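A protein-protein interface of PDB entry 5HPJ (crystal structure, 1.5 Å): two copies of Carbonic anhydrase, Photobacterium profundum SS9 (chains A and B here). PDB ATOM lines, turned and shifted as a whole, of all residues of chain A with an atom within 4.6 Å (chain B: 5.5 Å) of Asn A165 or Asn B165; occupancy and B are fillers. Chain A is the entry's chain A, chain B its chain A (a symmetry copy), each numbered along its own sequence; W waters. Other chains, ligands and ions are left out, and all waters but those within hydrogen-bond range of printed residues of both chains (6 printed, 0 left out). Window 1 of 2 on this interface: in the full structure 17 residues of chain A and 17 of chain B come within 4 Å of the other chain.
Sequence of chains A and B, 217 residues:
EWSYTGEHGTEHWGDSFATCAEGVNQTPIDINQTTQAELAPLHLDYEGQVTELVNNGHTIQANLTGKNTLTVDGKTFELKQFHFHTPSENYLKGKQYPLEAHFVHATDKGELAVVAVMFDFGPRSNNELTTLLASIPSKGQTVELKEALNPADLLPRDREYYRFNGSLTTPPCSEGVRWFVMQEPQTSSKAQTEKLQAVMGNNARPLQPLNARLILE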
ATOM      1  N   ASN A  25      17.524   7.154  15.847  1.00  0.00           N
ATOM      2  CA  ASN A  25      16.366   7.740  16.524  1.00  0.00           C
ATOM      3  C   ASN A  25      15.120   7.501  15.663  1.00  0.00           C
ATOM      4  O   ASN A  25      14.400   8.425  15.301  1.00  0.00           O
ATOM      5  CB  ASN A  25      16.608   9.226  16.758  1.00  0.00           C
ATOM      6  CG  ASN A  25      17.655   9.476  17.819  1.00  0.00           C
ATOM      7  OD1 ASN A  25      17.360   9.433  19.014  1.00  0.00           O
ATOM      8  ND2 ASN A  25      18.882   9.744  17.390  1.00  0.00           N
ATOM      9  N   PHE A 164       7.586  10.428  22.271  1.00  0.00           N
ATOM     10  CA  PHE A 164       8.992  10.183  21.995  1.00  0.00           C
ATOM     11  C   PHE A 164       9.436  10.940  20.755  1.00  0.00           C
ATOM     12  O   PHE A 164       8.617  11.460  19.991  1.00  0.00           O
ATOM     13  CB  PHE A 164       9.310   8.681  21.918  1.00  0.00           C
ATOM     14  CG  PHE A 164       8.637   7.954  20.791  1.00  0.00           C
ATOM     15  CD1 PHE A 164       9.303   7.756  19.592  1.00  0.00           C
ATOM     16  CD2 PHE A 164       7.357   7.440  20.937  1.00  0.00           C
ATOM     17  CE1 PHE A 164       8.696   7.071  18.547  1.00  0.00           C
ATOM     18  CE2 PHE A 164       6.742   6.764  19.895  1.00  0.00           C
ATOM     19  CZ  PHE A 164       7.406   6.570  18.716  1.00  0.00           C
ATOM     20  N   ASN A 165      10.755  11.014  20.607  1.00  0.00           N
ATOM     21  CA  ASN A 165      11.424  11.688  19.516  1.00  0.00           C
ATOM     22  C   ASN A 165      11.838  10.606  18.540  1.00  0.00           C
ATOM     23  O   ASN A 165      12.520   9.650  18.920  1.00  0.00           O
ATOM     24  CB  ASN A 165      12.615  12.419  20.119  1.00  0.00           C
ATOM     25  CG  ASN A 165      13.738  12.684  19.127  1.00  0.00           C
ATOM     26  OD1 ASN A 165      13.542  13.221  18.045  1.00  0.00           O
ATOM     27  ND2 ASN A 165      14.956  12.313  19.524  1.00  0.00           N
ATOM     28  N   GLY A 166      11.385  10.696  17.301  1.00  0.00           N
ATOM     29  CA  GLY A 166      11.672   9.653  16.339  1.00  0.00           C
ATOM     30  C   GLY A 166      11.741  10.142  14.903  1.00  0.00           C
ATOM     31  O   GLY A 166      12.329  11.185  14.614  1.00  0.00           O
ATOM     32  N   GLY A 176      13.999  13.912  13.777  1.00  0.00           N
ATOM     33  CA  GLY A 176      13.506  15.177  14.305  1.00  0.00           C
ATOM     34  C   GLY A 176      11.989  15.261  14.295  1.00  0.00           C
ATOM     35  O   GLY A 176      11.429  16.365  14.278  1.00  0.00           O
ATOM     36  N   VAL A 177      11.341  14.103  14.308  1.00  0.00           N
ATOM     37  CA  VAL A 177       9.877  14.017  14.253  1.00  0.00           C
ATOM     38  C   VAL A 177       9.325  13.728  15.640  1.00  0.00           C
ATOM     39  O   VAL A 177       9.705  12.757  16.279  1.00  0.00           O
ATOM     40  CB  VAL A 177       9.400  12.924  13.263  1.00  0.00           C
ATOM     41  CG1 VAL A 177       7.860  12.818  13.247  1.00  0.00           C
ATOM     42  CG2 VAL A 177       9.956  13.181  11.870  1.00  0.00           C
ATOM     43  N   ALA A 212      19.268   5.642  22.951  1.00  0.00           N
ATOM     44  CA  ALA A 212      19.475   6.507  24.110  1.00  0.00           C
ATOM     45  C   ALA A 212      18.214   7.256  24.558  1.00  0.00           C
ATOM     46  O   ALA A 212      18.237   7.999  25.540  1.00  0.00           O
ATOM     47  CB  ALA A 212      20.574   7.494  23.815  1.00  0.00           C
ATOM     48  N   ARG A 213      17.119   7.048  23.850  1.00  0.00           N
ATOM     49  CA  ARG A 213      15.861   7.719  24.144  1.00  0.00           C
ATOM     50  C   ARG A 213      15.151   7.156  25.358  1.00  0.00           C
ATOM     51  O   ARG A 213      15.307   5.986  25.693  1.00  0.00           O
ATOM     52  CB  ARG A 213      14.934   7.588  22.932  1.00  0.00           C
ATOM     53  CG  ARG A 213      15.488   8.260  21.692  1.00  0.00           C
ATOM     54  CD  ARG A 213      14.617   8.004  20.486  1.00  0.00           C
ATOM     55  NE  ARG A 213      14.752   6.640  19.994  1.00  0.00           N
ATOM     56  CZ  ARG A 213      14.071   6.155  18.966  1.00  0.00           C
ATOM     57  NH1 ARG A 213      13.191   6.929  18.328  1.00  0.00           N
ATOM     58  NH2 ARG A 213      14.257   4.911  18.565  1.00  0.00           N
ATOM     59  N   ASN B  25      19.920  15.182  16.245  1.00  0.00           N
ATOM     60  CA  ASN B  25      19.912  14.840  17.668  1.00  0.00           C
ATOM     61  C   ASN B  25      21.322  15.044  18.232  1.00  0.00           C
ATOM     62  O   ASN B  25      21.920  14.146  18.813  1.00  0.00           O
ATOM     63  CB  ASN B  25      19.441  13.402  17.846  1.00  0.00           C
ATOM     64  CG  ASN B  25      17.966  13.240  17.554  1.00  0.00           C
ATOM     65  OD1 ASN B  25      17.124  13.521  18.408  1.00  0.00           O
ATOM     66  ND2 ASN B  25      17.646  12.783  16.351  1.00  0.00           N
ATOM     67  N   GLN B  26      21.847  16.237  18.006  1.00  0.00           N
ATOM     68  CA  GLN B  26      23.230  16.554  18.322  1.00  0.00           C
ATOM     69  C   GLN B  26      23.418  17.256  19.659  1.00  0.00           C
ATOM     70  O   GLN B  26      22.501  17.834  20.216  1.00  0.00           O
ATOM     71  CB  GLN B  26      23.823  17.431  17.222  1.00  0.00           C
ATOM     72  CG  GLN B  26      23.906  16.768  15.851  1.00  0.00           C
ATOM     73  CD  GLN B  26      25.107  15.869  15.737  1.00  0.00           C
ATOM     74  OE1 GLN B  26      26.251  16.328  15.713  1.00  0.00           O
ATOM     75  NE2 GLN B  26      24.865  14.578  15.687  1.00  0.00           N
ATOM     76  N   THR B  27      24.648  17.156  20.163  1.00  0.00           N
ATOM     77  CA  THR B  27      25.128  17.860  21.349  1.00  0.00           C
ATOM     78  C   THR B  27      26.214  18.829  20.854  1.00  0.00           C
ATOM     79  O   THR B  27      26.935  18.502  19.912  1.00  0.00           O
ATOM     80  CB  THR B  27      25.695  16.845  22.351  1.00  0.00           C
ATOM     81  OG1 THR B  27      24.684  15.868  22.630  1.00  0.00           O
ATOM     82  CG2 THR B  27      26.142  17.493  23.659  1.00  0.00           C
ATOM     83  N   ARG B 163      19.023  15.048  31.811  1.00  0.00           N
ATOM     84  CA  ARG B 163      19.245  13.991  30.846  1.00  0.00           C
ATOM     85  C   ARG B 163      18.702  14.346  29.481  1.00  0.00           C
ATOM     86  O   ARG B 163      17.576  14.826  29.326  1.00  0.00           O
ATOM     87  CB  ARG B 163      18.609  12.677  31.303  1.00  0.00           C
ATOM     88  CG  ARG B 163      18.738  11.573  30.250  1.00  0.00           C
ATOM     89  CD  ARG B 163      18.079  10.271  30.653  1.00  0.00           C
ATOM     90  NE  ARG B 163      18.166   9.308  29.558  1.00  0.00           N
ATOM     91  CZ  ARG B 163      18.352   8.001  29.705  1.00  0.00           C
ATOM     92  NH1 ARG B 163      18.468   7.469  30.912  1.00  0.00           N
ATOM     93  NH2 ARG B 163      18.415   7.223  28.629  1.00  0.00           N
ATOM     94  N   PHE B 164      19.503  14.073  28.466  1.00  0.00           N
ATOM     95  CA  PHE B 164      19.009  14.127  27.100  1.00  0.00           C
ATOM     96  C   PHE B 164      19.740  13.124  26.224  1.00  0.00           C
ATOM     97  O   PHE B 164      20.767  12.560  26.612  1.00  0.00           O
ATOM     98  CB  PHE B 164      19.050  15.554  26.530  1.00  0.00           C
ATOM     99  CG  PHE B 164      20.428  16.134  26.389  1.00  0.00           C
ATOM    100  CD1 PHE B 164      21.099  16.052  25.180  1.00  0.00           C
ATOM    101  CD2 PHE B 164      21.037  16.787  27.449  1.00  0.00           C
ATOM    102  CE1 PHE B 164      22.367  16.598  25.034  1.00  0.00           C
ATOM    103  CE2 PHE B 164      22.307  17.327  27.313  1.00  0.00           C
ATOM    104  CZ  PHE B 164      22.962  17.244  26.116  1.00  0.00           C
ATOM    105  N   ASN B 165      19.154  12.897  25.053  1.00  0.00           N
ATOM    106  CA  ASN B 165      19.648  11.980  24.049  1.00  0.00           C
ATOM    107  C   ASN B 165      20.352  12.828  23.011  1.00  0.00           C
ATOM    108  O   ASN B 165      19.763  13.765  22.465  1.00  0.00           O
ATOM    109  CB  ASN B 165      18.434  11.254  23.487  1.00  0.00           C
ATOM    110  CG  ASN B 165      18.643  10.710  22.080  1.00  0.00           C
ATOM    111  OD1 ASN B 165      19.604  10.013  21.784  1.00  0.00           O
ATOM    112  ND2 ASN B 165      17.697  11.024  21.195  1.00  0.00           N
ATOM    113  N   GLY B 166      21.627  12.567  22.771  1.00  0.00           N
ATOM    114  CA  GLY B 166      22.384  13.390  21.853  1.00  0.00           C
ATOM    115  C   GLY B 166      23.506  12.653  21.145  1.00  0.00           C
ATOM    116  O   GLY B 166      23.333  11.523  20.686  1.00  0.00           O
ATOM    117  N   SER B 167      24.642  13.332  21.012  1.00  0.00           N
ATOM    118  CA  SER B 167      25.713  12.879  20.140  1.00  0.00           C
ATOM    119  C   SER B 167      27.056  13.155  20.768  1.00  0.00           C
ATOM    120  O   SER B 167      27.144  13.884  21.744  1.00  0.00           O
ATOM    121  CB  SER B 167      25.662  13.621  18.803  1.00  0.00           C
ATOM    122  OG  SER B 167      26.090  14.978  18.910  1.00  0.00           O
ATOM    123  N   GLY B 176      22.879   8.542  19.333  1.00  0.00           N
ATOM    124  CA  GLY B 176      22.576   7.443  20.239  1.00  0.00           C
ATOM    125  C   GLY B 176      23.385   7.508  21.524  1.00  0.00           C
ATOM    126  O   GLY B 176      23.591   6.478  22.180  1.00  0.00           O
ATOM    127  N   VAL B 177      23.833   8.707  21.872  1.00  0.00           N
ATOM    128  CA  VAL B 177      24.668   8.926  23.059  1.00  0.00           C
ATOM    129  C   VAL B 177      23.825   9.505  24.183  1.00  0.00           C
ATOM    130  O   VAL B 177      23.180  10.532  24.020  1.00  0.00           O
ATOM    131  CB  VAL B 177      25.861   9.868  22.759  1.00  0.00           C
ATOM    132  CG1 VAL B 177      26.706  10.120  24.026  1.00  0.00           C
ATOM    133  CG2 VAL B 177      26.710   9.318  21.622  1.00  0.00           C
ATOM    134  N   ARG B 178      23.789   8.816  25.310  1.00  0.00           N
ATOM    135  CA  ARG B 178      23.151   9.352  26.512  1.00  0.00           C
ATOM    136  C   ARG B 178      23.996  10.462  27.115  1.00  0.00           C
ATOM    137  O   ARG B 178      25.198  10.284  27.328  1.00  0.00           O
ATOM    138  CB  ARG B 178      22.995   8.255  27.557  1.00  0.00           C
ATOM    139  CG  ARG B 178      22.033   7.143  27.193  1.00  0.00           C
ATOM    140  CD  ARG B 178      22.396   5.902  27.978  1.00  0.00           C
ATOM    141  NE  ARG B 178      21.339   4.890  28.009  1.00  0.00           N
ATOM    142  CZ  ARG B 178      21.178   3.939  27.105  1.00  0.00           C
ATOM    143  NH1 ARG B 178      21.978   3.844  26.051  1.00  0.00           N
ATOM    144  NH2 ARG B 178      20.193   3.065  27.265  1.00  0.00           N
ATOM    145  N   TRP B 179      23.353  11.584  27.412  1.00  0.00           N
ATOM    146  CA  TRP B 179      23.977  12.708  28.097  1.00  0.00           C
ATOM    147  C   TRP B 179      23.360  12.937  29.466  1.00  0.00           C
ATOM    148  O   TRP B 179      22.136  13.050  29.608  1.00  0.00           O
ATOM    149  CB  TRP B 179      23.885  13.986  27.250  1.00  0.00           C
ATOM    150  CG  TRP B 179      24.942  13.976  26.189  1.00  0.00           C
ATOM    151  CD1 TRP B 179      24.916  13.300  24.990  1.00  0.00           C
ATOM    152  CD2 TRP B 179      26.214  14.621  26.250  1.00  0.00           C
ATOM    153  NE1 TRP B 179      26.096  13.501  24.310  1.00  0.00           N
ATOM    154  CE2 TRP B 179      26.912  14.299  25.062  1.00  0.00           C
ATOM    155  CE3 TRP B 179      26.832  15.446  27.185  1.00  0.00           C
ATOM    156  CZ2 TRP B 179      28.188  14.794  24.788  1.00  0.00           C
ATOM    157  CZ3 TRP B 179      28.097  15.918  26.912  1.00  0.00           C
ATOM    158  CH2 TRP B 179      28.753  15.602  25.732  1.00  0.00           C
ATOM    159  N   ALA B 212      13.168  17.740  18.159  1.00  0.00           N
ATOM    160  CA  ALA B 212      11.999  17.077  18.732  1.00  0.00           C
ATOM    161  C   ALA B 212      12.222  16.545  20.153  1.00  0.00           C
ATOM    162  O   ALA B 212      11.312  15.987  20.767  1.00  0.00           O
ATOM    163  CB  ALA B 212      11.565  15.952  17.830  1.00  0.00           C
ATOM    164  N   ARG B 213      13.421  16.730  20.672  1.00  0.00           N
ATOM    165  CA  ARG B 213      13.779  16.248  21.998  1.00  0.00           C
ATOM    166  C   ARG B 213      13.193  17.082  23.119  1.00  0.00           C
ATOM    167  O   ARG B 213      12.943  18.273  22.954  1.00  0.00           O
ATOM    168  CB  ARG B 213      15.305  16.254  22.132  1.00  0.00           C
ATOM    169  CG  ARG B 213      15.986  15.324  21.149  1.00  0.00           C
ATOM    170  CD  ARG B 213      17.489  15.448  21.217  1.00  0.00           C
ATOM    171  NE  ARG B 213      17.964  16.684  20.611  1.00  0.00           N
ATOM    172  CZ  ARG B 213      19.238  17.044  20.571  1.00  0.00           C
ATOM    173  NH1 ARG B 213      20.168  16.261  21.120  1.00  0.00           N
ATOM    174  NH2 ARG B 213      19.597  18.176  19.990  1.00  0.00           N
HETATM  175  O   HOH W   1      14.739  12.133  15.881  1.00  0.00           O
HETATM  176  O   HOH W   2      17.555  10.279  26.955  1.00  0.00           O
HETATM  177  O   HOH W   3      15.220  15.646  17.204  1.00  0.00           O
HETATM  178  O   HOH W   4      20.890  10.582  19.478  1.00  0.00           O
HETATM  179  O   HOH W   5      19.180   7.326  20.369  1.00  0.00           O
HETATM  180  O   HOH W   6      17.509   4.707  26.664  1.00  0.00           O
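The backbone carbonyl oxygen (O) of Ala A212 sits at hydrogen-bond distance from the guanidinium group (NH2) of Arg B163 (3.2 Å).
The side-chain amide nitrogen of Asn B25 sits close to the side-chain amide nitrogen of Asn A25 (3.4 Å).
The side-chain amide nitrogen (ND2) of Asn B165 lies close to the side-chain amide nitrogen (ND2) of Asn A165, 3.5 Å away.
The side-chain amide nitrogen of Asn B165 lies within hydrogen-bond range of the side-chain amide oxygen of Asn A25.
The side-chain amide nitrogen (ND2) of Asn A165 is in hydrogen-bond range of the side-chain amide oxygen (OD1) of Asn B25 (2.7 Å).
The backbone carbonyl oxygen (O) of Gly A166 sits at hydrogen-bond distance from the backbone NH (N) of Gly A176 (3.3 Å).
The backbone carbonyl oxygen (O) of Val A177 sits at hydrogen-bond distance from the backbone NH (N) of Gly A166.
O of Asn B165 lies within hydrogen-bond range of NH1 of Arg B213, 2.9 Å away.
NH2 of Arg B213 is in hydrogen-bond range of O of Gln B26 (2.9 Å).
The backbone carbonyl oxygen (O) of Val B177 is in hydrogen-bond range of the backbone NH (N) of Gly B166.
O of Asn A165 is in hydrogen-bond range of NH1 of Arg A213, at 2.9 Å.
Among the printed residues, pairs that only touch across the chains: Asn A165 with Ala B212, Asn A165 with Arg B213, Gly A176 with Ala B212, Val A177 with Ala B212, Ala A212 with Asn B165, Ala A212 with Gly B176, Ala A212 with Val B177, Ala A212 with Arg B178 and Arg A213 with Asn B165.
Printed residues of chain B within 4 Å of Asn A165: Asn B25 (2.7 Å), Asn B165 (3.5 Å), Ala B212 (3.4 Å) and Arg B213 (3.6 Å).
Asn B165 touches four residues of chain A.
Of the printed residues of chain A, Arg B213 touches Asn A165.
Printed residues of chain A within 4 Å of Arg B178: Ala A212 (3.7 Å).
Printed residues of chain A within 4 Å of Gly B176: Ala A212 (3.6 Å).
Printed residues of chain B within 4 Å of Arg A213: Asn B165.
Of the printed residues of chain A, Val B177 touches Ala A212 (3.8 Å).
Thr B27 touches none of the printed residues of chain A.
Gly A166 touches none of the printed residues of chain B.
The nearest printed residue of chain B that does not touch Asn A165 is Gly B166 (7.4 Å).
The nearest printed residue of chain A that does not touch Asn B165 is Gly A166 (7.4 Å).
The nearest printed residue of chain B that does not touch Asn A25 is Gly B176 (4.6 Å).
Of the 8 printed residues of chain A, 6 touch a printed residue of chain B.
Along chain A the printed residues that touch a printed residue of chain B span positions 25 to 213.
Of the 14 printed residues of chain B, 8 touch a printed residue of chain A.
Along chain B the printed residues that touch a printed residue of chain A span positions 25 to 213.
Among the printed residues, 14 pairs touch across the chains.
Among the printed residues, no Asp or Glu carboxylate lies within 4 Å of a Lys or Arg side-chain nitrogen of the other chain.
Asn A25 touches Asn B165, and with the chains exchanged Asn A165 touches Asn B25.
Asn A165 touches Ala B212, and with the chains exchanged Ala A212 touches Asn B165.
Asn A165 touches Arg B213, and with the chains exchanged Arg A213 touches Asn B165.
Val A177 touches Ala B212, and with the chains exchanged Ala A212 touches Val B177.
Positions printed for both chains: 25, 164, 165, 166, 176, 177, 212 and 213.
Of the 14 pairs that touch across the chains among the printed residues, 12 have their exchanged pair printed and touching as well.
Water W4 lies within hydrogen-bond range of the side-chain amide oxygen of Asn B165 (2.7 Å), the backbone NH of Gly B176 (2.9 Å), the backbone carbonyl oxygen of Gly B166 (2.9 Å) and the side-chain amide nitrogen of Asn A25 (3.0 Å).
Water W1 lies within hydrogen-bond range of the side-chain amide oxygen (OD1) of Asn A165 (2.7 Å), the backbone NH (N) of Gly A176 (2.9 Å), the backbone carbonyl oxygen (O) of Gly A166 (2.9 Å) and the side-chain amide nitrogen (ND2) of Asn B25 (3.0 Å).
Water W6 lies within hydrogen-bond range of the backbone carbonyl oxygen (O) of Arg A213 (2.7 Å), the guanidinium group (NH2) of Arg B178 (3.2 Å) and the guanidinium group (NH2) of Arg B163 (3.3 Å).
Water W2 lies within hydrogen-bond range of the backbone carbonyl oxygen of Ala A212 (2.8 Å) and the guanidinium group of Arg B163 (2.8 Å).
Water W5 lies within hydrogen-bond range of OD1 of Asn B165 (3.1 Å), N of Ala A212 (3.1 Å) and OD1 of Asn A25 (3.1 Å).
Water W3 lies within hydrogen-bond range of the side-chain amide oxygen of Asn A165, the backbone NH of Ala B212 and the side-chain amide oxygen of Asn B25.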
